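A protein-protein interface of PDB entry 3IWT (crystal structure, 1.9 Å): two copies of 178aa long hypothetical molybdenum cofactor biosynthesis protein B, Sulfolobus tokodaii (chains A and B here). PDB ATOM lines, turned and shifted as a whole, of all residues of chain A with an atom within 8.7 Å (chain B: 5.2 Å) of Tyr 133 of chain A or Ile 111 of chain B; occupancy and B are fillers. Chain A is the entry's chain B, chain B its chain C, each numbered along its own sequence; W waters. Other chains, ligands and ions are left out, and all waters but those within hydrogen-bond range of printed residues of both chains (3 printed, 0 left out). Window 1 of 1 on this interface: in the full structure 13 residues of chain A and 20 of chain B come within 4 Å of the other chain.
The backbone carbonyl oxygen of Tyr 93 of chain A sits at hydrogen-bond distance from the guanidinium group of Arg 109 of chain B (2.8 Å).
The backbone carbonyl oxygen (O) of Glu 110 of chain B lies within hydrogen-bond range of the side-chain hydroxyl (OH) of Tyr 93 of chain A, 3.5 Å away.
The side-chain hydroxyl of Tyr 93 of chain A lies within hydrogen-bond range of the backbone NH of Glu 112 of chain B, 2.9 Å away.
OH of Tyr 133 of chain A sits at hydrogen-bond distance from OH of Tyr 148 of chain B (2.9 Å).
The side-chain hydroxyl (OH) of Tyr 133 of chain A is in hydrogen-bond range of the backbone carbonyl oxygen (O) of Leu 164 of chain B (2.8 Å).
O of Thr 91 of chain A lies within hydrogen-bond range of N of Lys 136 of chain A (2.8 Å).
The backbone carbonyl oxygen (O) of Thr 135 of chain A sits at hydrogen-bond distance from the guanidinium group (NH1) of Arg 119 of chain A (3.1 Å).
The backbone carbonyl oxygen of Arg 109 of chain B is in hydrogen-bond range of the backbone NH of Ile 141 of chain B, at 2.9 Å.
The backbone carbonyl oxygen (O) of Ala 139 of chain B sits at hydrogen-bond distance from the backbone NH (N) of Ile 111 of chain B (2.8 Å).
Among the printed residues, merely in contact across the chains: Arg 119 of chain A with Gly 113 of chain B, Tyr 93 of chain A with Ile 111 of chain B, Leu 134 of chain A with Glu 168 of chain B, Tyr 133 of chain A with Ile 111 of chain B, Tyr 133 of chain A with Gly 113 of chain B, Leu 134 of chain A with Leu 172 of chain B, Ala 131 of chain A with Glu 168 of chain B, Tyr 133 of chain A with Phe 114 of chain B, Tyr 93 of chain A with Ile 141 of chain B, Tyr 133 of chain A with Glu 168 of chain B, Phe 123 of chain A with Val 117 of chain B, Ala 130 of chain A with Glu 168 of chain B, Ala 130 of chain A with Leu 164 of chain B, Tyr 133 of chain A with Val 117 of chain B and Lys 136 of chain A with Glu 112 of chain B.
Ile 111 of chain B touches just these residues of chain A: Tyr 93 (3.3 Å) and Tyr 133 (3.4 Å).
Gly 113 of chain B touches just these residues of chain A: Arg 119 and Tyr 133.
No residue of chain A comes within 4 Å of Gly 140 of chain B.
Of the printed residues of chain A, Ile 141 of chain B touches Tyr 93 (3.7 Å).
Printed residues of chain B within 4 Å of Ala 130 of chain A: Leu 164 and Glu 168.
The nearest residue of chain A that does not touch Ile 111 of chain B is Leu 134 of chain A (4.8 Å).
The nearest printed residue of chain B that does not touch Ala 130 of chain A is Val 117 of chain B (5.1 Å).
Printed residues of chain A that touch a printed residue of chain B: Tyr 93, Arg 119, Phe 123, Ala 130, Ala 131, Tyr 133, Leu 134 and Lys 136.
Hydrophobic or aromatic side chains of chain A within 4 Å of the printed part of chain B: Tyr 93, Phe 123, Ala 130, Ala 131, Tyr 133 and Leu 134.
Along chain A the printed residues that touch a printed residue of chain B span positions 93 to 136.
Printed residues of chain B that touch a printed residue of chain A: Arg 109, Glu 110, Ile 111, Glu 112, Gly 113, Phe 114, Val 117, Ile 141, Tyr 148, Leu 164, Glu 168 and Leu 172.
Among the printed residues, no Asp or Glu carboxylate lies within 4 Å of a Lys or Arg side-chain nitrogen of the other chain.
1 position is printed for both chains.
Water W1 lies within hydrogen-bond range of the side-chain carboxylate of Glu 112 of chain B (2.6 Å), the guanidinium group of Arg 119 of chain A (2.8 Å) and the side-chain hydroxyl of Ser 115 of chain A (3.5 Å).
Water W3 lies within hydrogen-bond range of the side-chain hydroxyl of Tyr 93 of chain A (2.6 Å), the backbone carbonyl oxygen of Tyr 133 of chain A (2.7 Å), the backbone carbonyl oxygen of Thr 135 of chain A (2.8 Å) and the backbone NH of Gly 113 of chain B (2.9 Å).
Water W2 lies within hydrogen-bond range of the backbone carbonyl oxygen of Glu 110 of chain B and the side-chain amino group of Lys 136 of chain A.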
ATOM      1  N   THR A  91      16.383 -40.656 -17.396  1.00  0.00           N
ATOM      2  CA  THR A  91      15.339 -39.967 -16.640  1.00  0.00           C
ATOM      3  C   THR A  91      14.875 -38.634 -17.293  1.00  0.00           C
ATOM      4  O   THR A  91      14.228 -37.814 -16.630  1.00  0.00           O
ATOM      5  CB  THR A  91      15.785 -39.728 -15.163  1.00  0.00           C
ATOM      6  OG1 THR A  91      16.888 -38.805 -15.124  1.00  0.00           O
ATOM      7  CG2 THR A  91      16.173 -41.031 -14.483  1.00  0.00           C
ATOM      8  N   GLY A  92      15.215 -38.403 -18.563  1.00  0.00           N
ATOM      9  CA  GLY A  92      14.833 -37.169 -19.255  1.00  0.00           C
ATOM     10  C   GLY A  92      13.745 -37.419 -20.299  1.00  0.00           C
ATOM     11  O   GLY A  92      12.947 -38.341 -20.166  1.00  0.00           O
ATOM     12  N   TYR A  93      13.718 -36.572 -21.334  1.00  0.00           N
ATOM     13  CA  TYR A  93      12.654 -36.572 -22.316  1.00  0.00           C
ATOM     14  C   TYR A  93      13.134 -36.996 -23.714  1.00  0.00           C
ATOM     15  O   TYR A  93      12.441 -36.800 -24.707  1.00  0.00           O
ATOM     16  CB  TYR A  93      11.938 -35.217 -22.347  1.00  0.00           C
ATOM     17  CG  TYR A  93      11.219 -34.977 -21.047  1.00  0.00           C
ATOM     18  CD1 TYR A  93       9.962 -35.498 -20.833  1.00  0.00           C
ATOM     19  CD2 TYR A  93      11.838 -34.289 -20.014  1.00  0.00           C
ATOM     20  CE1 TYR A  93       9.325 -35.330 -19.638  1.00  0.00           C
ATOM     21  CE2 TYR A  93      11.201 -34.086 -18.808  1.00  0.00           C
ATOM     22  CZ  TYR A  93       9.955 -34.624 -18.624  1.00  0.00           C
ATOM     23  OH  TYR A  93       9.304 -34.458 -17.436  1.00  0.00           O
ATOM     24  N   SER A 115      11.721 -35.661  -6.407  1.00  0.00           N
ATOM     25  CA  SER A 115      11.701 -35.063  -7.740  1.00  0.00           C
ATOM     26  C   SER A 115      11.829 -33.535  -7.724  1.00  0.00           C
ATOM     27  O   SER A 115      12.735 -32.967  -8.339  1.00  0.00           O
ATOM     28  CB  SER A 115      10.429 -35.484  -8.465  1.00  0.00           C
ATOM     29  OG  SER A 115      10.443 -36.886  -8.643  1.00  0.00           O
ATOM     30  N   PHE A 118      15.062 -32.249  -5.971  1.00  0.00           N
ATOM     31  CA  PHE A 118      16.211 -32.370  -6.868  1.00  0.00           C
ATOM     32  C   PHE A 118      16.193 -31.270  -7.950  1.00  0.00           C
ATOM     33  O   PHE A 118      17.222 -30.712  -8.278  1.00  0.00           O
ATOM     34  CB  PHE A 118      16.311 -33.749  -7.526  1.00  0.00           C
ATOM     35  CG  PHE A 118      17.476 -33.850  -8.466  1.00  0.00           C
ATOM     36  CD1 PHE A 118      18.776 -33.792  -7.985  1.00  0.00           C
ATOM     37  CD2 PHE A 118      17.270 -33.921  -9.828  1.00  0.00           C
ATOM     38  CE1 PHE A 118      19.876 -33.840  -8.866  1.00  0.00           C
ATOM     39  CE2 PHE A 118      18.352 -33.985 -10.707  1.00  0.00           C
ATOM     40  CZ  PHE A 118      19.665 -33.916 -10.221  1.00  0.00           C
ATOM     41  N   ARG A 119      15.007 -30.948  -8.470  1.00  0.00           N
ATOM     42  CA  ARG A 119      14.883 -29.907  -9.461  1.00  0.00           C
ATOM     43  C   ARG A 119      15.172 -28.516  -8.877  1.00  0.00           C
ATOM     44  O   ARG A 119      15.691 -27.654  -9.584  1.00  0.00           O
ATOM     45  CB  ARG A 119      13.529 -29.955 -10.140  1.00  0.00           C
ATOM     46  CG  ARG A 119      13.394 -31.140 -11.071  1.00  0.00           C
ATOM     47  CD  ARG A 119      12.083 -31.098 -11.860  1.00  0.00           C
ATOM     48  NE  ARG A 119      10.872 -31.428 -11.080  1.00  0.00           N
ATOM     49  CZ  ARG A 119      10.238 -32.594 -11.092  1.00  0.00           C
ATOM     50  NH1 ARG A 119      10.709 -33.613 -11.762  1.00  0.00           N
ATOM     51  NH2 ARG A 119       9.109 -32.758 -10.410  1.00  0.00           N
ATOM     52  N   LEU A 120      14.852 -28.326  -7.596  1.00  0.00           N
ATOM     53  CA  LEU A 120      15.165 -27.087  -6.879  1.00  0.00           C
ATOM     54  C   LEU A 120      16.683 -26.857  -6.797  1.00  0.00           C
ATOM     55  O   LEU A 120      17.184 -25.777  -7.170  1.00  0.00           O
ATOM     56  CB  LEU A 120      14.510 -27.141  -5.489  1.00  0.00           C
ATOM     57  CG  LEU A 120      14.694 -26.037  -4.445  1.00  0.00           C
ATOM     58  CD1 LEU A 120      13.649 -26.292  -3.367  1.00  0.00           C
ATOM     59  CD2 LEU A 120      16.062 -26.076  -3.849  1.00  0.00           C
ATOM     60  N   SER A 122      18.963 -28.307  -8.595  1.00  0.00           N
ATOM     61  CA  SER A 122      19.456 -28.233  -9.977  1.00  0.00           C
ATOM     62  C   SER A 122      19.229 -26.841 -10.549  1.00  0.00           C
ATOM     63  O   SER A 122      20.147 -26.243 -11.103  1.00  0.00           O
ATOM     64  CB  SER A 122      18.734 -29.269 -10.866  1.00  0.00           C
ATOM     65  OG  SER A 122      19.080 -30.592 -10.481  1.00  0.00           O
ATOM     66  N   PHE A 123      18.031 -26.295 -10.360  1.00  0.00           N
ATOM     67  CA  PHE A 123      17.701 -24.956 -10.863  1.00  0.00           C
ATOM     68  C   PHE A 123      18.653 -23.904 -10.308  1.00  0.00           C
ATOM     69  O   PHE A 123      19.007 -22.969 -11.002  1.00  0.00           O
ATOM     70  CB  PHE A 123      16.290 -24.519 -10.466  1.00  0.00           C
ATOM     71  CG  PHE A 123      15.883 -23.200 -11.073  1.00  0.00           C
ATOM     72  CD1 PHE A 123      15.442 -23.126 -12.388  1.00  0.00           C
ATOM     73  CD2 PHE A 123      15.987 -22.031 -10.348  1.00  0.00           C
ATOM     74  CE1 PHE A 123      15.116 -21.884 -12.964  1.00  0.00           C
ATOM     75  CE2 PHE A 123      15.671 -20.807 -10.921  1.00  0.00           C
ATOM     76  CZ  PHE A 123      15.224 -20.755 -12.225  1.00  0.00           C
ATOM     77  N   VAL A 128      22.721 -24.781 -14.934  1.00  0.00           N
ATOM     78  CA  VAL A 128      21.575 -25.646 -15.226  1.00  0.00           C
ATOM     79  C   VAL A 128      20.346 -24.778 -15.340  1.00  0.00           C
ATOM     80  O   VAL A 128      19.743 -24.709 -16.407  1.00  0.00           O
ATOM     81  CB  VAL A 128      21.407 -26.758 -14.164  1.00  0.00           C
ATOM     82  CG1 VAL A 128      20.096 -27.585 -14.417  1.00  0.00           C
ATOM     83  CG2 VAL A 128      22.674 -27.653 -14.136  1.00  0.00           C
ATOM     84  N   LYS A 129      19.987 -24.088 -14.266  1.00  0.00           N
ATOM     85  CA  LYS A 129      18.860 -23.166 -14.276  1.00  0.00           C
ATOM     86  C   LYS A 129      17.609 -23.865 -14.847  1.00  0.00           C
ATOM     87  O   LYS A 129      17.269 -24.942 -14.383  1.00  0.00           O
ATOM     88  CB  LYS A 129      19.208 -21.817 -14.968  1.00  0.00           C
ATOM     89  CG  LYS A 129      20.291 -21.002 -14.205  1.00  0.00           C
ATOM     90  CD  LYS A 129      20.394 -19.590 -14.757  1.00  0.00           C
ATOM     91  CE  LYS A 129      21.621 -18.827 -14.224  1.00  0.00           C
ATOM     92  NZ  LYS A 129      21.675 -17.449 -14.752  1.00  0.00           N
ATOM     93  N   ALA A 130      16.994 -23.299 -15.881  1.00  0.00           N
ATOM     94  CA  ALA A 130      15.734 -23.792 -16.421  1.00  0.00           C
ATOM     95  C   ALA A 130      15.795 -25.218 -16.975  1.00  0.00           C
ATOM     96  O   ALA A 130      14.771 -25.877 -17.028  1.00  0.00           O
ATOM     97  CB  ALA A 130      15.201 -22.829 -17.489  1.00  0.00           C
ATOM     98  N   ALA A 131      16.986 -25.689 -17.353  1.00  0.00           N
ATOM     99  CA  ALA A 131      17.177 -27.094 -17.716  1.00  0.00           C
ATOM    100  C   ALA A 131      16.665 -28.035 -16.616  1.00  0.00           C
ATOM    101  O   ALA A 131      16.381 -29.209 -16.908  1.00  0.00           O
ATOM    102  CB  ALA A 131      18.644 -27.391 -18.017  1.00  0.00           C
ATOM    103  N   ALA A 132      16.498 -27.518 -15.389  1.00  0.00           N
ATOM    104  CA  ALA A 132      15.991 -28.328 -14.270  1.00  0.00           C
ATOM    105  C   ALA A 132      14.651 -28.991 -14.573  1.00  0.00           C
ATOM    106  O   ALA A 132      14.367 -30.064 -14.041  1.00  0.00           O
ATOM    107  CB  ALA A 132      15.883 -27.522 -13.004  1.00  0.00           C
ATOM    108  N   TYR A 133      13.804 -28.379 -15.392  1.00  0.00           N
ATOM    109  CA  TYR A 133      12.492 -28.977 -15.639  1.00  0.00           C
ATOM    110  C   TYR A 133      12.489 -30.082 -16.654  1.00  0.00           C
ATOM    111  O   TYR A 133      11.434 -30.689 -16.886  1.00  0.00           O
ATOM    112  CB  TYR A 133      11.398 -27.947 -15.909  1.00  0.00           C
ATOM    113  CG  TYR A 133      11.333 -27.238 -17.252  1.00  0.00           C
ATOM    114  CD1 TYR A 133      10.678 -27.808 -18.358  1.00  0.00           C
ATOM    115  CD2 TYR A 133      11.813 -25.950 -17.383  1.00  0.00           C
ATOM    116  CE1 TYR A 133      10.564 -27.136 -19.567  1.00  0.00           C
ATOM    117  CE2 TYR A 133      11.701 -25.251 -18.583  1.00  0.00           C
ATOM    118  CZ  TYR A 133      11.089 -25.842 -19.677  1.00  0.00           C
ATOM    119  OH  TYR A 133      10.970 -25.121 -20.839  1.00  0.00           O
ATOM    120  N   LEU A 134      13.655 -30.358 -17.236  1.00  0.00           N
ATOM    121  CA  LEU A 134      13.827 -31.439 -18.196  1.00  0.00           C
ATOM    122  C   LEU A 134      14.276 -32.778 -17.575  1.00  0.00           C
ATOM    123  O   LEU A 134      14.592 -33.717 -18.298  1.00  0.00           O
ATOM    124  CB  LEU A 134      14.819 -30.987 -19.285  1.00  0.00           C
ATOM    125  CG  LEU A 134      14.420 -29.745 -20.108  1.00  0.00           C
ATOM    126  CD1 LEU A 134      15.387 -29.616 -21.295  1.00  0.00           C
ATOM    127  CD2 LEU A 134      13.020 -29.781 -20.580  1.00  0.00           C
ATOM    128  N   THR A 135      14.282 -32.881 -16.244  1.00  0.00           N
ATOM    129  CA  THR A 135      14.565 -34.159 -15.559  1.00  0.00           C
ATOM    130  C   THR A 135      13.369 -34.669 -14.750  1.00  0.00           C
ATOM    131  O   THR A 135      12.562 -33.878 -14.241  1.00  0.00           O
ATOM    132  CB  THR A 135      15.799 -34.055 -14.621  1.00  0.00           C
ATOM    133  OG1 THR A 135      16.121 -35.369 -14.145  1.00  0.00           O
ATOM    134  CG2 THR A 135      15.543 -33.115 -13.422  1.00  0.00           C
ATOM    135  N   LYS A 136      13.258 -35.992 -14.669  1.00  0.00           N
ATOM    136  CA  LYS A 136      12.270 -36.687 -13.865  1.00  0.00           C
ATOM    137  C   LYS A 136      12.943 -37.564 -12.806  1.00  0.00           C
ATOM    138  O   LYS A 136      12.328 -38.534 -12.353  1.00  0.00           O
ATOM    139  CB  LYS A 136      11.393 -37.585 -14.755  1.00  0.00           C
ATOM    140  CG  LYS A 136      10.581 -36.855 -15.788  1.00  0.00           C
ATOM    141  CD  LYS A 136       9.746 -37.804 -16.663  1.00  0.00           C
ATOM    142  CE  LYS A 136      10.591 -38.387 -17.791  1.00  0.00           C
ATOM    143  NZ  LYS A 136       9.714 -39.017 -18.808  1.00  0.00           N
ATOM    144  N   ALA A 137      14.188 -37.246 -12.414  1.00  0.00           N
ATOM    145  CA  ALA A 137      14.858 -37.985 -11.326  1.00  0.00           C
ATOM    146  C   ALA A 137      13.864 -38.162 -10.161  1.00  0.00           C
ATOM    147  O   ALA A 137      13.162 -37.220  -9.813  1.00  0.00           O
ATOM    148  CB  ALA A 137      16.161 -37.273 -10.844  1.00  0.00           C
ATOM    149  N   ARG B 109       3.334 -37.438 -22.976  1.00  0.00           N
ATOM    150  CA  ARG B 109       4.175 -37.395 -21.779  1.00  0.00           C
ATOM    151  C   ARG B 109       4.018 -36.008 -21.133  1.00  0.00           C
ATOM    152  O   ARG B 109       4.096 -34.996 -21.818  1.00  0.00           O
ATOM    153  CB  ARG B 109       5.654 -37.611 -22.134  1.00  0.00           C
ATOM    154  CG  ARG B 109       5.965 -38.953 -22.809  1.00  0.00           C
ATOM    155  CD  ARG B 109       7.476 -39.193 -22.921  1.00  0.00           C
ATOM    156  NE  ARG B 109       8.084 -38.410 -23.995  1.00  0.00           N
ATOM    157  CZ  ARG B 109       9.385 -38.425 -24.294  1.00  0.00           C
ATOM    158  NH1 ARG B 109      10.235 -39.177 -23.590  1.00  0.00           N
ATOM    159  NH2 ARG B 109       9.832 -37.690 -25.305  1.00  0.00           N
ATOM    160  N   GLU B 110       3.770 -35.981 -19.824  1.00  0.00           N
ATOM    161  CA  GLU B 110       3.760 -34.721 -19.089  1.00  0.00           C
ATOM    162  C   GLU B 110       5.211 -34.340 -18.800  1.00  0.00           C
ATOM    163  O   GLU B 110       6.049 -35.184 -18.430  1.00  0.00           O
ATOM    164  CB  GLU B 110       2.991 -34.813 -17.770  1.00  0.00           C
ATOM    165  CG  GLU B 110       3.105 -33.538 -16.992  1.00  0.00           C
ATOM    166  CD  GLU B 110       1.950 -33.268 -16.074  1.00  0.00           C
ATOM    167  OE1 GLU B 110       1.407 -34.239 -15.499  1.00  0.00           O
ATOM    168  OE2 GLU B 110       1.571 -32.060 -15.971  1.00  0.00           O
ATOM    169  N   ILE B 111       5.524 -33.076 -19.001  1.00  0.00           N
ATOM    170  CA  ILE B 111       6.834 -32.577 -18.596  1.00  0.00           C
ATOM    171  C   ILE B 111       6.650 -32.193 -17.134  1.00  0.00           C
ATOM    172  O   ILE B 111       6.285 -31.049 -16.785  1.00  0.00           O
ATOM    173  CB  ILE B 111       7.333 -31.406 -19.481  1.00  0.00           C
ATOM    174  CG1 ILE B 111       7.511 -31.878 -20.926  1.00  0.00           C
ATOM    175  CG2 ILE B 111       8.668 -30.892 -18.933  1.00  0.00           C
ATOM    176  CD1 ILE B 111       7.602 -30.760 -21.960  1.00  0.00           C
ATOM    177  N   GLU B 112       6.914 -33.175 -16.283  1.00  0.00           N
ATOM    178  CA  GLU B 112       6.436 -33.157 -14.899  1.00  0.00           C
ATOM    179  C   GLU B 112       6.973 -31.975 -14.081  1.00  0.00           C
ATOM    180  O   GLU B 112       6.259 -31.342 -13.307  1.00  0.00           O
ATOM    181  CB  GLU B 112       6.810 -34.491 -14.220  1.00  0.00           C
ATOM    182  CG  GLU B 112       6.204 -35.744 -14.907  1.00  0.00           C
ATOM    183  CD  GLU B 112       6.646 -37.055 -14.271  1.00  0.00           C
ATOM    184  OE1 GLU B 112       7.477 -37.029 -13.333  1.00  0.00           O
ATOM    185  OE2 GLU B 112       6.164 -38.123 -14.720  1.00  0.00           O
ATOM    186  N   GLY B 113       8.224 -31.672 -14.299  1.00  0.00           N
ATOM    187  CA  GLY B 113       8.927 -30.658 -13.523  1.00  0.00           C
ATOM    188  C   GLY B 113       8.640 -29.238 -13.927  1.00  0.00           C
ATOM    189  O   GLY B 113       9.043 -28.315 -13.228  1.00  0.00           O
ATOM    190  N   PHE B 114       7.957 -29.014 -15.052  1.00  0.00           N
ATOM    191  CA  PHE B 114       7.618 -27.634 -15.426  1.00  0.00           C
ATOM    192  C   PHE B 114       6.755 -26.974 -14.325  1.00  0.00           C
ATOM    193  O   PHE B 114       6.958 -25.823 -13.985  1.00  0.00           O
ATOM    194  CB  PHE B 114       6.898 -27.528 -16.793  1.00  0.00           C
ATOM    195  CG  PHE B 114       6.601 -26.095 -17.178  1.00  0.00           C
ATOM    196  CD1 PHE B 114       7.574 -25.309 -17.769  1.00  0.00           C
ATOM    197  CD2 PHE B 114       5.366 -25.526 -16.886  1.00  0.00           C
ATOM    198  CE1 PHE B 114       7.312 -23.961 -18.087  1.00  0.00           C
ATOM    199  CE2 PHE B 114       5.084 -24.197 -17.202  1.00  0.00           C
ATOM    200  CZ  PHE B 114       6.071 -23.405 -17.786  1.00  0.00           C
ATOM    201  N   SER B 115       5.804 -27.729 -13.777  1.00  0.00           N
ATOM    202  CA  SER B 115       4.904 -27.216 -12.754  1.00  0.00           C
ATOM    203  C   SER B 115       5.627 -26.682 -11.523  1.00  0.00           C
ATOM    204  O   SER B 115       5.435 -25.519 -11.135  1.00  0.00           O
ATOM    205  CB  SER B 115       3.907 -28.299 -12.362  1.00  0.00           C
ATOM    206  OG  SER B 115       3.124 -28.611 -13.487  1.00  0.00           O
ATOM    207  N   VAL B 117       8.983 -26.177 -11.095  1.00  0.00           N
ATOM    208  CA  VAL B 117      10.017 -25.188 -11.395  1.00  0.00           C
ATOM    209  C   VAL B 117       9.360 -23.821 -11.688  1.00  0.00           C
ATOM    210  O   VAL B 117       9.889 -22.791 -11.296  1.00  0.00           O
ATOM    211  CB  VAL B 117      10.939 -25.657 -12.548  1.00  0.00           C
ATOM    212  CG1 VAL B 117      11.959 -24.543 -12.952  1.00  0.00           C
ATOM    213  CG2 VAL B 117      11.699 -26.929 -12.094  1.00  0.00           C
ATOM    214  N   ALA B 139       3.203 -28.294 -18.530  1.00  0.00           N
ATOM    215  CA  ALA B 139       3.758 -28.511 -19.873  1.00  0.00           C
ATOM    216  C   ALA B 139       3.746 -30.008 -20.208  1.00  0.00           C
ATOM    217  O   ALA B 139       3.787 -30.903 -19.326  1.00  0.00           O
ATOM    218  CB  ALA B 139       5.192 -27.955 -20.006  1.00  0.00           C
ATOM    219  N   GLY B 140       3.687 -30.279 -21.505  1.00  0.00           N
ATOM    220  CA  GLY B 140       3.696 -31.640 -21.990  1.00  0.00           C
ATOM    221  C   GLY B 140       4.091 -31.761 -23.429  1.00  0.00           C
ATOM    222  O   GLY B 140       4.361 -30.764 -24.084  1.00  0.00           O
ATOM    223  N   ILE B 141       4.087 -33.005 -23.918  1.00  0.00           N
ATOM    224  CA  ILE B 141       4.529 -33.355 -25.267  1.00  0.00           C
ATOM    225  C   ILE B 141       3.367 -34.127 -25.925  1.00  0.00           C
ATOM    226  O   ILE B 141       2.790 -35.016 -25.301  1.00  0.00           O
ATOM    227  CB  ILE B 141       5.822 -34.241 -25.211  1.00  0.00           C
ATOM    228  CG1 ILE B 141       6.970 -33.512 -24.495  1.00  0.00           C
ATOM    229  CG2 ILE B 141       6.244 -34.712 -26.607  1.00  0.00           C
ATOM    230  CD1 ILE B 141       8.010 -34.440 -23.832  1.00  0.00           C
ATOM    231  N   ILE B 146       5.445 -29.481 -28.493  1.00  0.00           N
ATOM    232  CA  ILE B 146       5.505 -29.136 -27.083  1.00  0.00           C
ATOM    233  C   ILE B 146       4.315 -28.249 -26.761  1.00  0.00           C
ATOM    234  O   ILE B 146       3.918 -27.397 -27.573  1.00  0.00           O
ATOM    235  CB  ILE B 146       6.802 -28.363 -26.734  1.00  0.00           C
ATOM    236  CG1 ILE B 146       8.056 -29.108 -27.224  1.00  0.00           C
ATOM    237  CG2 ILE B 146       6.888 -28.119 -25.213  1.00  0.00           C
ATOM    238  CD1 ILE B 146       8.214 -30.520 -26.693  1.00  0.00           C
ATOM    239  N   TYR B 148       2.685 -25.729 -23.611  1.00  0.00           N
ATOM    240  CA  TYR B 148       2.792 -25.024 -22.317  1.00  0.00           C
ATOM    241  C   TYR B 148       1.432 -24.423 -21.975  1.00  0.00           C
ATOM    242  O   TYR B 148       0.869 -23.659 -22.759  1.00  0.00           O
ATOM    243  CB  TYR B 148       3.850 -23.917 -22.360  1.00  0.00           C
ATOM    244  CG  TYR B 148       5.287 -24.352 -22.556  1.00  0.00           C
ATOM    245  CD1 TYR B 148       6.077 -24.730 -21.479  1.00  0.00           C
ATOM    246  CD2 TYR B 148       5.859 -24.370 -23.831  1.00  0.00           C
ATOM    247  CE1 TYR B 148       7.407 -25.133 -21.664  1.00  0.00           C
ATOM    248  CE2 TYR B 148       7.175 -24.767 -24.024  1.00  0.00           C
ATOM    249  CZ  TYR B 148       7.963 -25.106 -22.936  1.00  0.00           C
ATOM    250  OH  TYR B 148       9.277 -25.460 -23.148  1.00  0.00           O
ATOM    251  N   LEU B 164      11.761 -19.696 -18.361  1.00  0.00           N
ATOM    252  CA  LEU B 164      11.657 -21.159 -18.572  1.00  0.00           C
ATOM    253  C   LEU B 164      11.472 -21.591 -20.021  1.00  0.00           C
ATOM    254  O   LEU B 164      12.088 -22.577 -20.435  1.00  0.00           O
ATOM    255  CB  LEU B 164      10.547 -21.774 -17.707  1.00  0.00           C
ATOM    256  CG  LEU B 164      10.639 -21.552 -16.182  1.00  0.00           C
ATOM    257  CD1 LEU B 164       9.513 -22.369 -15.499  1.00  0.00           C
ATOM    258  CD2 LEU B 164      12.017 -21.942 -15.602  1.00  0.00           C
ATOM    259  N   ILE B 165      10.639 -20.882 -20.787  1.00  0.00           N
ATOM    260  CA  ILE B 165      10.333 -21.315 -22.154  1.00  0.00           C
ATOM    261  C   ILE B 165      11.437 -20.915 -23.121  1.00  0.00           C
ATOM    262  O   ILE B 165      12.093 -21.786 -23.715  1.00  0.00           O
ATOM    263  CB  ILE B 165       8.912 -20.823 -22.629  1.00  0.00           C
ATOM    264  CG1 ILE B 165       7.847 -21.382 -21.688  1.00  0.00           C
ATOM    265  CG2 ILE B 165       8.647 -21.188 -24.086  1.00  0.00           C
ATOM    266  CD1 ILE B 165       6.476 -20.851 -21.919  1.00  0.00           C
ATOM    267  N   GLU B 168      14.919 -22.897 -22.963  1.00  0.00           N
ATOM    268  CA  GLU B 168      14.983 -24.368 -23.092  1.00  0.00           C
ATOM    269  C   GLU B 168      14.155 -24.962 -24.208  1.00  0.00           C
ATOM    270  O   GLU B 168      14.331 -26.139 -24.543  1.00  0.00           O
ATOM    271  CB  GLU B 168      14.639 -25.066 -21.766  1.00  0.00           C
ATOM    272  CG  GLU B 168      15.815 -25.090 -20.776  1.00  0.00           C
ATOM    273  CD  GLU B 168      17.070 -25.753 -21.345  1.00  0.00           C
ATOM    274  OE1 GLU B 168      16.953 -26.714 -22.152  1.00  0.00           O
ATOM    275  OE2 GLU B 168      18.183 -25.303 -20.989  1.00  0.00           O
ATOM    276  N   VAL B 169      13.269 -24.180 -24.813  1.00  0.00           N
ATOM    277  CA  VAL B 169      12.306 -24.763 -25.747  1.00  0.00           C
ATOM    278  C   VAL B 169      12.982 -25.343 -27.008  1.00  0.00           C
ATOM    279  O   VAL B 169      12.553 -26.371 -27.512  1.00  0.00           O
ATOM    280  CB  VAL B 169      11.138 -23.788 -26.107  1.00  0.00           C
ATOM    281  CG1 VAL B 169      11.647 -22.558 -26.877  1.00  0.00           C
ATOM    282  CG2 VAL B 169      10.037 -24.569 -26.856  1.00  0.00           C
ATOM    283  N   LEU B 172      14.424 -28.739 -26.083  1.00  0.00           N
ATOM    284  CA  LEU B 172      13.334 -29.662 -25.856  1.00  0.00           C
ATOM    285  C   LEU B 172      12.691 -30.129 -27.187  1.00  0.00           C
ATOM    286  O   LEU B 172      12.447 -31.327 -27.380  1.00  0.00           O
ATOM    287  CB  LEU B 172      12.332 -28.992 -24.909  1.00  0.00           C
ATOM    288  CG  LEU B 172      11.148 -29.766 -24.376  1.00  0.00           C
ATOM    289  CD1 LEU B 172      11.519 -31.080 -23.629  1.00  0.00           C
ATOM    290  CD2 LEU B 172      10.382 -28.759 -23.479  1.00  0.00           C
HETATM  291  O   HOH W   1       9.241 -35.989 -11.789  1.00  0.00           O
HETATM  292  O   HOH W   2       6.646 -37.772 -18.496  1.00  0.00           O
HETATM  293  O   HOH W   3      10.462 -32.871 -15.728  1.00  0.00           O
